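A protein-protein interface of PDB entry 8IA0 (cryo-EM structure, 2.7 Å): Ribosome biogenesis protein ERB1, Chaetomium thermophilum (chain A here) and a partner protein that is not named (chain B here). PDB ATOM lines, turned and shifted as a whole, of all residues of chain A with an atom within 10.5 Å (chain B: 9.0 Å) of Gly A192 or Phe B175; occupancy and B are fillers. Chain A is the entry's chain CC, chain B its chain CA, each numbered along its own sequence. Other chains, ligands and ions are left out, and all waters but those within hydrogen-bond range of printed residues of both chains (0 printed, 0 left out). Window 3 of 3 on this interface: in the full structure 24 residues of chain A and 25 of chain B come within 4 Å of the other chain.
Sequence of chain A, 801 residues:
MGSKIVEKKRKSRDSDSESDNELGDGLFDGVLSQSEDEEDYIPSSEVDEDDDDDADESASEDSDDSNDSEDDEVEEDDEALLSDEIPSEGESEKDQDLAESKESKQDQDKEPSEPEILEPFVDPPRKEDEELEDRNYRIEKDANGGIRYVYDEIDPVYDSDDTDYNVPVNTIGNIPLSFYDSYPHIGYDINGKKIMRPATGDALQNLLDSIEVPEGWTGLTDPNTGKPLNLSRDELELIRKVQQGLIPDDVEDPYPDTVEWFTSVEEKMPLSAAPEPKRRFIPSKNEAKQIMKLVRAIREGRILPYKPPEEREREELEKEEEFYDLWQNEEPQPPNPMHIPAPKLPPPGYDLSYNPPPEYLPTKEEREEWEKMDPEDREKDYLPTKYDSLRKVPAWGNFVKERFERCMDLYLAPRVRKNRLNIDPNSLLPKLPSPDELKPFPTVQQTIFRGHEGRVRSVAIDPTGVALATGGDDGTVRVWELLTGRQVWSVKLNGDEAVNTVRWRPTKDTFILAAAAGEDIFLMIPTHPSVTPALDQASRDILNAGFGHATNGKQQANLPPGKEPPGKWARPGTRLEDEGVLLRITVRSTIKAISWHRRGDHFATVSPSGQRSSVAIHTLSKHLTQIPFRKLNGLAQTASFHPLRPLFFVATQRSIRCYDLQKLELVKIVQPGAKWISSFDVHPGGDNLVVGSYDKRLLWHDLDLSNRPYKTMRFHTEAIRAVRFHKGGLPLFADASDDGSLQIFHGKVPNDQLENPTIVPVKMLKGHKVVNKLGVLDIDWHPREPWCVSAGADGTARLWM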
ATOM      1  N   VAL A 169      17.973  10.899  22.745  1.00  0.00           N
ATOM      2  CA  VAL A 169      16.565  11.171  23.009  1.00  0.00           C
ATOM      3  C   VAL A 169      15.793  11.477  21.731  1.00  0.00           C
ATOM      4  O   VAL A 169      14.557  11.515  21.752  1.00  0.00           O
ATOM      5  CB  VAL A 169      16.434  12.339  24.002  1.00  0.00           C
ATOM      6  CG1 VAL A 169      15.061  12.355  24.655  1.00  0.00           C
ATOM      7  CG2 VAL A 169      17.526  12.261  25.052  1.00  0.00           C
ATOM      8  N   ASN A 170      16.488  11.675  20.610  1.00  0.00           N
ATOM      9  CA  ASN A 170      15.827  12.161  19.404  1.00  0.00           C
ATOM     10  C   ASN A 170      14.953  11.099  18.751  1.00  0.00           C
ATOM     11  O   ASN A 170      14.027  11.443  18.009  1.00  0.00           O
ATOM     12  CB  ASN A 170      16.863  12.671  18.407  1.00  0.00           C
ATOM     13  CG  ASN A 170      16.246  13.513  17.311  1.00  0.00           C
ATOM     14  OD1 ASN A 170      15.111  13.968  17.431  1.00  0.00           O
ATOM     15  ND2 ASN A 170      16.994  13.730  16.237  1.00  0.00           N
ATOM     16  N   THR A 171      15.239   9.818  18.991  1.00  0.00           N
ATOM     17  CA  THR A 171      14.474   8.714  18.402  1.00  0.00           C
ATOM     18  C   THR A 171      14.427   8.847  16.878  1.00  0.00           C
ATOM     19  O   THR A 171      13.477   8.433  16.212  1.00  0.00           O
ATOM     20  CB  THR A 171      13.068   8.638  19.004  1.00  0.00           C
ATOM     21  OG1 THR A 171      13.155   8.792  20.425  1.00  0.00           O
ATOM     22  CG2 THR A 171      12.426   7.294  18.722  1.00  0.00           C
ATOM     23  N   ILE A 172      15.472   9.443  16.320  1.00  0.00           N
ATOM     24  CA  ILE A 172      15.610   9.629  14.884  1.00  0.00           C
ATOM     25  C   ILE A 172      16.818   8.824  14.439  1.00  0.00           C
ATOM     26  O   ILE A 172      17.912   8.982  14.992  1.00  0.00           O
ATOM     27  CB  ILE A 172      15.767  11.116  14.516  1.00  0.00           C
ATOM     28  CG1 ILE A 172      14.437  11.848  14.693  1.00  0.00           C
ATOM     29  CG2 ILE A 172      16.281  11.270  13.098  1.00  0.00           C
ATOM     30  CD1 ILE A 172      13.259  11.100  14.130  1.00  0.00           C
ATOM     31  N   TYR A 180      13.018  18.086   8.597  1.00  0.00           N
ATOM     32  CA  TYR A 180      12.870  18.981   9.743  1.00  0.00           C
ATOM     33  C   TYR A 180      13.566  20.318   9.536  1.00  0.00           C
ATOM     34  O   TYR A 180      13.603  21.126  10.469  1.00  0.00           O
ATOM     35  CB  TYR A 180      13.389  18.381  11.060  1.00  0.00           C
ATOM     36  CG  TYR A 180      12.822  17.032  11.434  1.00  0.00           C
ATOM     37  CD1 TYR A 180      11.669  16.930  12.191  1.00  0.00           C
ATOM     38  CD2 TYR A 180      13.459  15.861  11.056  1.00  0.00           C
ATOM     39  CE1 TYR A 180      11.155  15.704  12.546  1.00  0.00           C
ATOM     40  CE2 TYR A 180      12.952  14.631  11.406  1.00  0.00           C
ATOM     41  CZ  TYR A 180      11.802  14.559  12.152  1.00  0.00           C
ATOM     42  OH  TYR A 180      11.291  13.333  12.502  1.00  0.00           O
ATOM     43  N   HIS A 185      10.207  21.860  15.077  1.00  0.00           N
ATOM     44  CA  HIS A 185      10.648  20.756  15.913  1.00  0.00           C
ATOM     45  C   HIS A 185      11.722  19.947  15.200  1.00  0.00           C
ATOM     46  O   HIS A 185      11.889  20.024  13.981  1.00  0.00           O
ATOM     47  CB  HIS A 185       9.471  19.847  16.279  1.00  0.00           C
ATOM     48  CG  HIS A 185       8.909  19.093  15.116  1.00  0.00           C
ATOM     49  ND1 HIS A 185       9.036  17.728  14.983  1.00  0.00           N
ATOM     50  CD2 HIS A 185       8.219  19.514  14.031  1.00  0.00           C
ATOM     51  CE1 HIS A 185       8.448  17.340  13.867  1.00  0.00           C
ATOM     52  NE2 HIS A 185       7.946  18.404  13.269  1.00  0.00           N
ATOM     53  N   GLY A 187      12.593  16.053  15.425  1.00  0.00           N
ATOM     54  CA  GLY A 187      12.380  14.699  15.895  1.00  0.00           C
ATOM     55  C   GLY A 187      11.251  14.566  16.902  1.00  0.00           C
ATOM     56  O   GLY A 187      10.595  15.527  17.302  1.00  0.00           O
ATOM     57  N   TYR A 188      11.037  13.320  17.320  1.00  0.00           N
ATOM     58  CA  TYR A 188      10.030  12.951  18.306  1.00  0.00           C
ATOM     59  C   TYR A 188      10.689  12.114  19.390  1.00  0.00           C
ATOM     60  O   TYR A 188      11.599  11.337  19.104  1.00  0.00           O
ATOM     61  CB  TYR A 188       8.899  12.140  17.672  1.00  0.00           C
ATOM     62  CG  TYR A 188       7.756  12.950  17.119  1.00  0.00           C
ATOM     63  CD1 TYR A 188       7.857  13.580  15.887  1.00  0.00           C
ATOM     64  CD2 TYR A 188       6.568  13.067  17.819  1.00  0.00           C
ATOM     65  CE1 TYR A 188       6.809  14.313  15.375  1.00  0.00           C
ATOM     66  CE2 TYR A 188       5.517  13.797  17.317  1.00  0.00           C
ATOM     67  CZ  TYR A 188       5.642  14.417  16.095  1.00  0.00           C
ATOM     68  OH  TYR A 188       4.590  15.147  15.595  1.00  0.00           O
ATOM     69  N   ASP A 189      10.231  12.259  20.629  1.00  0.00           N
ATOM     70  CA  ASP A 189      10.724  11.381  21.679  1.00  0.00           C
ATOM     71  C   ASP A 189       9.945  10.066  21.660  1.00  0.00           C
ATOM     72  O   ASP A 189       9.049   9.856  20.839  1.00  0.00           O
ATOM     73  CB  ASP A 189      10.654  12.069  23.042  1.00  0.00           C
ATOM     74  CG  ASP A 189       9.288  12.649  23.345  1.00  0.00           C
ATOM     75  OD1 ASP A 189       8.268  11.990  23.056  1.00  0.00           O
ATOM     76  OD2 ASP A 189       9.234  13.775  23.881  1.00  0.00           O
ATOM     77  N   ILE A 190      10.287   9.159  22.579  1.00  0.00           N
ATOM     78  CA  ILE A 190       9.654   7.844  22.600  1.00  0.00           C
ATOM     79  C   ILE A 190       8.249   7.867  23.176  1.00  0.00           C
ATOM     80  O   ILE A 190       7.557   6.844  23.129  1.00  0.00           O
ATOM     81  CB  ILE A 190      10.507   6.831  23.389  1.00  0.00           C
ATOM     82  CG1 ILE A 190      10.925   7.410  24.739  1.00  0.00           C
ATOM     83  CG2 ILE A 190      11.726   6.419  22.582  1.00  0.00           C
ATOM     84  CD1 ILE A 190      11.352   6.363  25.738  1.00  0.00           C
ATOM     85  N   ASN A 191       7.809   8.996  23.718  1.00  0.00           N
ATOM     86  CA  ASN A 191       6.456   9.127  24.240  1.00  0.00           C
ATOM     87  C   ASN A 191       5.480   9.690  23.218  1.00  0.00           C
ATOM     88  O   ASN A 191       4.297   9.853  23.538  1.00  0.00           O
ATOM     89  CB  ASN A 191       6.455  10.013  25.488  1.00  0.00           C
ATOM     90  CG  ASN A 191       7.207   9.390  26.642  1.00  0.00           C
ATOM     91  OD1 ASN A 191       6.953   8.247  27.018  1.00  0.00           O
ATOM     92  ND2 ASN A 191       8.143  10.140  27.211  1.00  0.00           N
ATOM     93  N   GLY A 192       5.935   9.991  22.007  1.00  0.00           N
ATOM     94  CA  GLY A 192       5.076  10.550  20.988  1.00  0.00           C
ATOM     95  C   GLY A 192       5.012  12.059  20.956  1.00  0.00           C
ATOM     96  O   GLY A 192       4.181  12.610  20.223  1.00  0.00           O
ATOM     97  N   LYS A 193       5.855  12.745  21.720  1.00  0.00           N
ATOM     98  CA  LYS A 193       5.887  14.199  21.761  1.00  0.00           C
ATOM     99  C   LYS A 193       7.096  14.705  20.986  1.00  0.00           C
ATOM    100  O   LYS A 193       8.175  14.111  21.044  1.00  0.00           O
ATOM    101  CB  LYS A 193       5.937  14.700  23.205  1.00  0.00           C
ATOM    102  CG  LYS A 193       5.320  16.073  23.408  1.00  0.00           C
ATOM    103  CD  LYS A 193       5.659  16.646  24.777  1.00  0.00           C
ATOM    104  CE  LYS A 193       7.081  16.304  25.198  1.00  0.00           C
ATOM    105  NZ  LYS A 193       7.707  17.405  25.980  1.00  0.00           N
ATOM    106  N   LYS A 194       6.909  15.798  20.254  1.00  0.00           N
ATOM    107  CA  LYS A 194       7.969  16.319  19.404  1.00  0.00           C
ATOM    108  C   LYS A 194       8.964  17.143  20.210  1.00  0.00           C
ATOM    109  O   LYS A 194       8.585  17.921  21.088  1.00  0.00           O
ATOM    110  CB  LYS A 194       7.382  17.166  18.276  1.00  0.00           C
ATOM    111  CG  LYS A 194       6.203  18.023  18.687  1.00  0.00           C
ATOM    112  CD  LYS A 194       5.831  19.004  17.592  1.00  0.00           C
ATOM    113  CE  LYS A 194       5.176  18.300  16.420  1.00  0.00           C
ATOM    114  NZ  LYS A 194       4.551  19.264  15.478  1.00  0.00           N
ATOM    115  N   ILE A 195      10.243  16.961  19.905  1.00  0.00           N
ATOM    116  CA  ILE A 195      11.315  17.724  20.532  1.00  0.00           C
ATOM    117  C   ILE A 195      11.505  19.015  19.753  1.00  0.00           C
ATOM    118  O   ILE A 195      11.724  18.992  18.536  1.00  0.00           O
ATOM    119  CB  ILE A 195      12.618  16.910  20.574  1.00  0.00           C
ATOM    120  CG1 ILE A 195      12.381  15.554  21.234  1.00  0.00           C
ATOM    121  CG2 ILE A 195      13.702  17.681  21.306  1.00  0.00           C
ATOM    122  CD1 ILE A 195      13.426  14.531  20.896  1.00  0.00           C
ATOM    123  N   MET A 196      11.429  20.142  20.450  1.00  0.00           N
ATOM    124  CA  MET A 196      11.492  21.441  19.801  1.00  0.00           C
ATOM    125  C   MET A 196      12.930  21.934  19.719  1.00  0.00           C
ATOM    126  O   MET A 196      13.782  21.568  20.533  1.00  0.00           O
ATOM    127  CB  MET A 196      10.632  22.458  20.551  1.00  0.00           C
ATOM    128  CG  MET A 196       9.258  21.939  20.944  1.00  0.00           C
ATOM    129  SD  MET A 196       8.069  21.877  19.586  1.00  0.00           S
ATOM    130  CE  MET A 196       8.624  23.236  18.561  1.00  0.00           C
ATOM    131  N   CYS B 132       7.772   0.012   7.543  1.00  0.00           N
ATOM    132  CA  CYS B 132       7.414   0.356   8.911  1.00  0.00           C
ATOM    133  C   CYS B 132       8.622   0.963   9.609  1.00  0.00           C
ATOM    134  O   CYS B 132       9.755   0.875   9.130  1.00  0.00           O
ATOM    135  CB  CYS B 132       6.902  -0.861   9.683  1.00  0.00           C
ATOM    136  SG  CYS B 132       8.191  -1.922  10.365  1.00  0.00           S
ATOM    137  N   LEU B 133       8.359   1.588  10.752  1.00  0.00           N
ATOM    138  CA  LEU B 133       9.417   2.214  11.531  1.00  0.00           C
ATOM    139  C   LEU B 133      10.372   1.163  12.084  1.00  0.00           C
ATOM    140  O   LEU B 133       9.960   0.072  12.483  1.00  0.00           O
ATOM    141  CB  LEU B 133       8.818   3.033  12.671  1.00  0.00           C
ATOM    142  CG  LEU B 133       8.376   4.459  12.348  1.00  0.00           C
ATOM    143  CD1 LEU B 133       7.169   4.845  13.181  1.00  0.00           C
ATOM    144  CD2 LEU B 133       9.514   5.428  12.583  1.00  0.00           C
ATOM    145  N   LYS B 134      11.656   1.503  12.104  1.00  0.00           N
ATOM    146  CA  LYS B 134      12.691   0.590  12.572  1.00  0.00           C
ATOM    147  C   LYS B 134      12.783   0.687  14.087  1.00  0.00           C
ATOM    148  O   LYS B 134      13.319   1.660  14.625  1.00  0.00           O
ATOM    149  CB  LYS B 134      14.024   0.924  11.910  1.00  0.00           C
ATOM    150  CG  LYS B 134      15.174   0.026  12.309  1.00  0.00           C
ATOM    151  CD  LYS B 134      16.480   0.538  11.740  1.00  0.00           C
ATOM    152  CE  LYS B 134      17.612  -0.433  12.003  1.00  0.00           C
ATOM    153  NZ  LYS B 134      17.781  -0.698  13.458  1.00  0.00           N
ATOM    154  N   GLY B 135      12.266  -0.324  14.778  1.00  0.00           N
ATOM    155  CA  GLY B 135      12.229  -0.331  16.224  1.00  0.00           C
ATOM    156  C   GLY B 135      10.885   0.000  16.831  1.00  0.00           C
ATOM    157  O   GLY B 135      10.768   0.002  18.062  1.00  0.00           O
ATOM    158  N   SER B 136       9.872   0.276  16.018  1.00  0.00           N
ATOM    159  CA  SER B 136       8.546   0.556  16.542  1.00  0.00           C
ATOM    160  C   SER B 136       7.957  -0.687  17.196  1.00  0.00           C
ATOM    161  O   SER B 136       8.242  -1.819  16.800  1.00  0.00           O
ATOM    162  CB  SER B 136       7.624   1.049  15.431  1.00  0.00           C
ATOM    163  OG  SER B 136       7.185  -0.026  14.620  1.00  0.00           O
ATOM    164  N   ARG B 137       7.137  -0.466  18.209  1.00  0.00           N
ATOM    165  CA  ARG B 137       6.549  -1.574  18.947  1.00  0.00           C
ATOM    166  C   ARG B 137       5.476  -2.246  18.105  1.00  0.00           C
ATOM    167  O   ARG B 137       4.528  -1.577  17.676  1.00  0.00           O
ATOM    168  CB  ARG B 137       5.966  -1.084  20.264  1.00  0.00           C
ATOM    169  CG  ARG B 137       6.994  -0.497  21.206  1.00  0.00           C
ATOM    170  CD  ARG B 137       6.511  -0.555  22.638  1.00  0.00           C
ATOM    171  NE  ARG B 137       6.079  -1.897  23.007  1.00  0.00           N
ATOM    172  CZ  ARG B 137       5.089  -2.161  23.848  1.00  0.00           C
ATOM    173  NH1 ARG B 137       4.396  -1.193  24.424  1.00  0.00           N
ATOM    174  NH2 ARG B 137       4.790  -3.426  24.119  1.00  0.00           N
ATOM    175  N   PRO B 138       5.575  -3.542  17.845  1.00  0.00           N
ATOM    176  CA  PRO B 138       4.607  -4.215  16.982  1.00  0.00           C
ATOM    177  C   PRO B 138       3.421  -4.767  17.762  1.00  0.00           C
ATOM    178  O   PRO B 138       3.450  -4.908  18.985  1.00  0.00           O
ATOM    179  CB  PRO B 138       5.433  -5.355  16.381  1.00  0.00           C
ATOM    180  CG  PRO B 138       6.396  -5.704  17.464  1.00  0.00           C
ATOM    181  CD  PRO B 138       6.654  -4.450  18.268  1.00  0.00           C
ATOM    182  N   SER B 172      13.232   2.283  20.983  1.00  0.00           N
ATOM    183  CA  SER B 172      12.046   2.025  20.189  1.00  0.00           C
ATOM    184  C   SER B 172      11.514   3.322  19.584  1.00  0.00           C
ATOM    185  O   SER B 172      12.044   4.410  19.810  1.00  0.00           O
ATOM    186  CB  SER B 172      10.973   1.354  21.041  1.00  0.00           C
ATOM    187  OG  SER B 172      10.553   2.206  22.090  1.00  0.00           O
ATOM    188  N   LYS B 173      10.432   3.192  18.798  1.00  0.00           N
ATOM    189  CA  LYS B 173       9.797   4.331  18.154  1.00  0.00           C
ATOM    190  C   LYS B 173       8.436   4.612  18.779  1.00  0.00           C
ATOM    191  O   LYS B 173       7.766   3.698  19.266  1.00  0.00           O
ATOM    192  CB  LYS B 173       9.627   4.080  16.654  1.00  0.00           C
ATOM    193  CG  LYS B 173      10.927   3.803  15.930  1.00  0.00           C
ATOM    194  CD  LYS B 173      11.773   5.054  15.845  1.00  0.00           C
ATOM    195  CE  LYS B 173      13.125   4.765  15.223  1.00  0.00           C
ATOM    196  NZ  LYS B 173      13.004   4.455  13.779  1.00  0.00           N
ATOM    197  N   PRO B 174       7.999   5.874  18.773  1.00  0.00           N
ATOM    198  CA  PRO B 174       6.803   6.231  19.549  1.00  0.00           C
ATOM    199  C   PRO B 174       5.492   5.759  18.945  1.00  0.00           C
ATOM    200  O   PRO B 174       4.537   5.527  19.696  1.00  0.00           O
ATOM    201  CB  PRO B 174       6.873   7.761  19.608  1.00  0.00           C
ATOM    202  CG  PRO B 174       7.679   8.146  18.426  1.00  0.00           C
ATOM    203  CD  PRO B 174       8.690   7.063  18.248  1.00  0.00           C
ATOM    204  N   PHE B 175       5.402   5.607  17.628  1.00  0.00           N
ATOM    205  CA  PHE B 175       4.134   5.328  16.969  1.00  0.00           C
ATOM    206  C   PHE B 175       4.139   3.926  16.375  1.00  0.00           C
ATOM    207  O   PHE B 175       5.171   3.445  15.897  1.00  0.00           O
ATOM    208  CB  PHE B 175       3.845   6.373  15.889  1.00  0.00           C
ATOM    209  CG  PHE B 175       3.856   7.780  16.406  1.00  0.00           C
ATOM    210  CD1 PHE B 175       2.758   8.293  17.069  1.00  0.00           C
ATOM    211  CD2 PHE B 175       4.974   8.579  16.256  1.00  0.00           C
ATOM    212  CE1 PHE B 175       2.768   9.580  17.557  1.00  0.00           C
ATOM    213  CE2 PHE B 175       4.991   9.866  16.747  1.00  0.00           C
ATOM    214  CZ  PHE B 175       3.886  10.368  17.397  1.00  0.00           C
ATOM    215  N   ILE B 176       2.978   3.279  16.409  1.00  0.00           N
ATOM    216  CA  ILE B 176       2.839   1.871  16.057  1.00  0.00           C
ATOM    217  C   ILE B 176       2.192   1.757  14.684  1.00  0.00           C
ATOM    218  O   ILE B 176       1.109   2.308  14.449  1.00  0.00           O
ATOM    219  CB  ILE B 176       2.026   1.119  17.123  1.00  0.00           C
ATOM    220  CG1 ILE B 176       1.535  -0.222  16.586  1.00  0.00           C
ATOM    221  CG2 ILE B 176       0.877   1.973  17.621  1.00  0.00           C
ATOM    222  CD1 ILE B 176       0.834  -1.042  17.623  1.00  0.00           C
ATOM    223  N   ASP B 177       2.857   1.039  13.772  1.00  0.00           N
ATOM    224  CA  ASP B 177       2.411   0.991  12.387  1.00  0.00           C
ATOM    225  C   ASP B 177       2.554  -0.378  11.727  1.00  0.00           C
ATOM    226  O   ASP B 177       2.295  -0.488  10.522  1.00  0.00           O
ATOM    227  CB  ASP B 177       3.174   2.028  11.558  1.00  0.00           C
ATOM    228  CG  ASP B 177       4.672   1.932  11.747  1.00  0.00           C
ATOM    229  OD1 ASP B 177       5.111   1.678  12.888  1.00  0.00           O
ATOM    230  OD2 ASP B 177       5.411   2.112  10.759  1.00  0.00           O
ATOM    231  N   HIS B 178       2.956  -1.420  12.451  1.00  0.00           N
ATOM    232  CA  HIS B 178       3.094  -2.727  11.824  1.00  0.00           C
ATOM    233  C   HIS B 178       2.695  -3.821  12.800  1.00  0.00           C
ATOM    234  O   HIS B 178       2.778  -3.651  14.018  1.00  0.00           O
ATOM    235  CB  HIS B 178       4.520  -2.964  11.311  1.00  0.00           C
ATOM    236  CG  HIS B 178       5.498  -3.349  12.375  1.00  0.00           C
ATOM    237  ND1 HIS B 178       5.928  -2.471  13.345  1.00  0.00           N
ATOM    238  CD2 HIS B 178       6.140  -4.517  12.613  1.00  0.00           C
ATOM    239  CE1 HIS B 178       6.788  -3.083  14.140  1.00  0.00           C
ATOM    240  NE2 HIS B 178       6.934  -4.325  13.716  1.00  0.00           N
ATOM    241  N   ILE B 196       0.360  -1.628   9.019  1.00  0.00           N
ATOM    242  CA  ILE B 196      -0.970  -1.126   9.335  1.00  0.00           C
ATOM    243  C   ILE B 196      -1.167   0.176   8.569  1.00  0.00           C
ATOM    244  O   ILE B 196      -0.658   1.226   8.968  1.00  0.00           O
ATOM    245  CB  ILE B 196      -1.149  -0.923  10.843  1.00  0.00           C
ATOM    246  CG1 ILE B 196      -0.860  -2.226  11.588  1.00  0.00           C
ATOM    247  CG2 ILE B 196      -2.552  -0.434  11.148  1.00  0.00           C
ATOM    248  CD1 ILE B 196      -1.134  -2.153  13.073  1.00  0.00           C
ATOM    249  N   GLU B 198      -3.777   3.002   7.304  1.00  0.00           N
ATOM    250  CA  GLU B 198      -5.076   3.565   7.639  1.00  0.00           C
ATOM    251  C   GLU B 198      -5.649   4.306   6.439  1.00  0.00           C
ATOM    252  O   GLU B 198      -4.943   5.077   5.780  1.00  0.00           O
ATOM    253  CB  GLU B 198      -4.959   4.503   8.837  1.00  0.00           C
ATOM    254  CG  GLU B 198      -4.680   3.791  10.144  1.00  0.00           C
ATOM    255  CD  GLU B 198      -4.354   4.750  11.269  1.00  0.00           C
ATOM    256  OE1 GLU B 198      -3.450   5.590  11.087  1.00  0.00           O
ATOM    257  OE2 GLU B 198      -5.002   4.665  12.333  1.00  0.00           O
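The backbone carbonyl oxygen (O) of Gly B135 is in hydrogen-bond range of the backbone NH (N) of Lys B173 (3.3 Å). OG1 of Thr A171 lies within hydrogen-bond range of O of Val A169 (3.3 Å). The backbone carbonyl oxygen (O) of Tyr A188 lies close to the backbone carbonyl oxygen (O) of Asn A170. The backbone carbonyl oxygen (O) of Tyr A188 lies close to the side-chain hydroxyl (OG1) of Thr A171 (3.3 Å). The side-chain carboxylate (OD1) of Asp A189 is in hydrogen-bond range of the backbone NH (N) of Asn A191 (3.1 Å). The side-chain carboxylate of Asp A189 is in hydrogen-bond range of the backbone NH of Gly A192, at 3.2 Å.
Of the printed residues of chain B, Thr A171 touches Ser B172 (3.1 Å), Lys B173 (3.7 Å) and Pro B174 (3.8 Å). Of the printed residues of chain B, Tyr A188 touches Phe B175. Printed residues of chain B within 4 Å of Asp A189: Pro B174 (3.3 Å). Of the printed residues of chain B, Ile A190 touches Ser B172 (3.4 Å) and Pro B174 (3.7 Å). Gly A192 touches just these residues of chain B: Pro B174 (3.4 Å) and Phe B175 (3.6 Å). No residue of chain A comes within 4 Å of Ser B136. Of the printed residues of chain A, Lys B173 touches Thr A171 (3.7 Å). Pro B174 touches just these residues of chain A: Thr A171 (3.8 Å), Asp A189 (3.3 Å), Ile A190 (3.7 Å) and Gly A192 (3.4 Å). Phe B175 touches just these residues of chain A: Tyr A188 and Gly A192. Ile B176 touches none of the printed residues of chain A. The nearest residue of chain B that does not touch Gly A192 is Lys B173 (6.8 Å). The nearest printed residue of chain A that does not touch Lys B173 is Ile A190 (5.0 Å).
Printed residues of chain B that touch a printed residue of chain A: Ser B172, Lys B173, Pro B174 and Phe B175. Hydrophobic or aromatic side chains of chain B that line the printed part of chain A: Pro B174 and Phe B175. Of the 16 printed residues of chain A, 5 touch a printed residue of chain B. Printed residues of chain A that touch a printed residue of chain B: Thr A171, Tyr A188, Asp A189, Ile A190 and Gly A192. Hydrophobic or aromatic side chains of chain A that line the printed part of chain B: Tyr A188 and Ile A190. Among the printed residues, 9 pairs touch across the chains.
Among the printed residues, pairs that only touch across the chains: Thr A171 with Ser B172 (3.1 Å), Asp A189 with Pro B174 (3.3 Å), Gly A192 with Pro B174 (3.4 Å), Ile A190 with Ser B172 (3.4 Å), Gly A192 with Phe B175 (3.6 Å), Ile A190 with Pro B174 (3.7 Å), Thr A171 with Lys B173 (3.7 Å), Tyr A188 with Phe B175 (3.7 Å) and Thr A171 with Pro B174 (3.8 Å).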
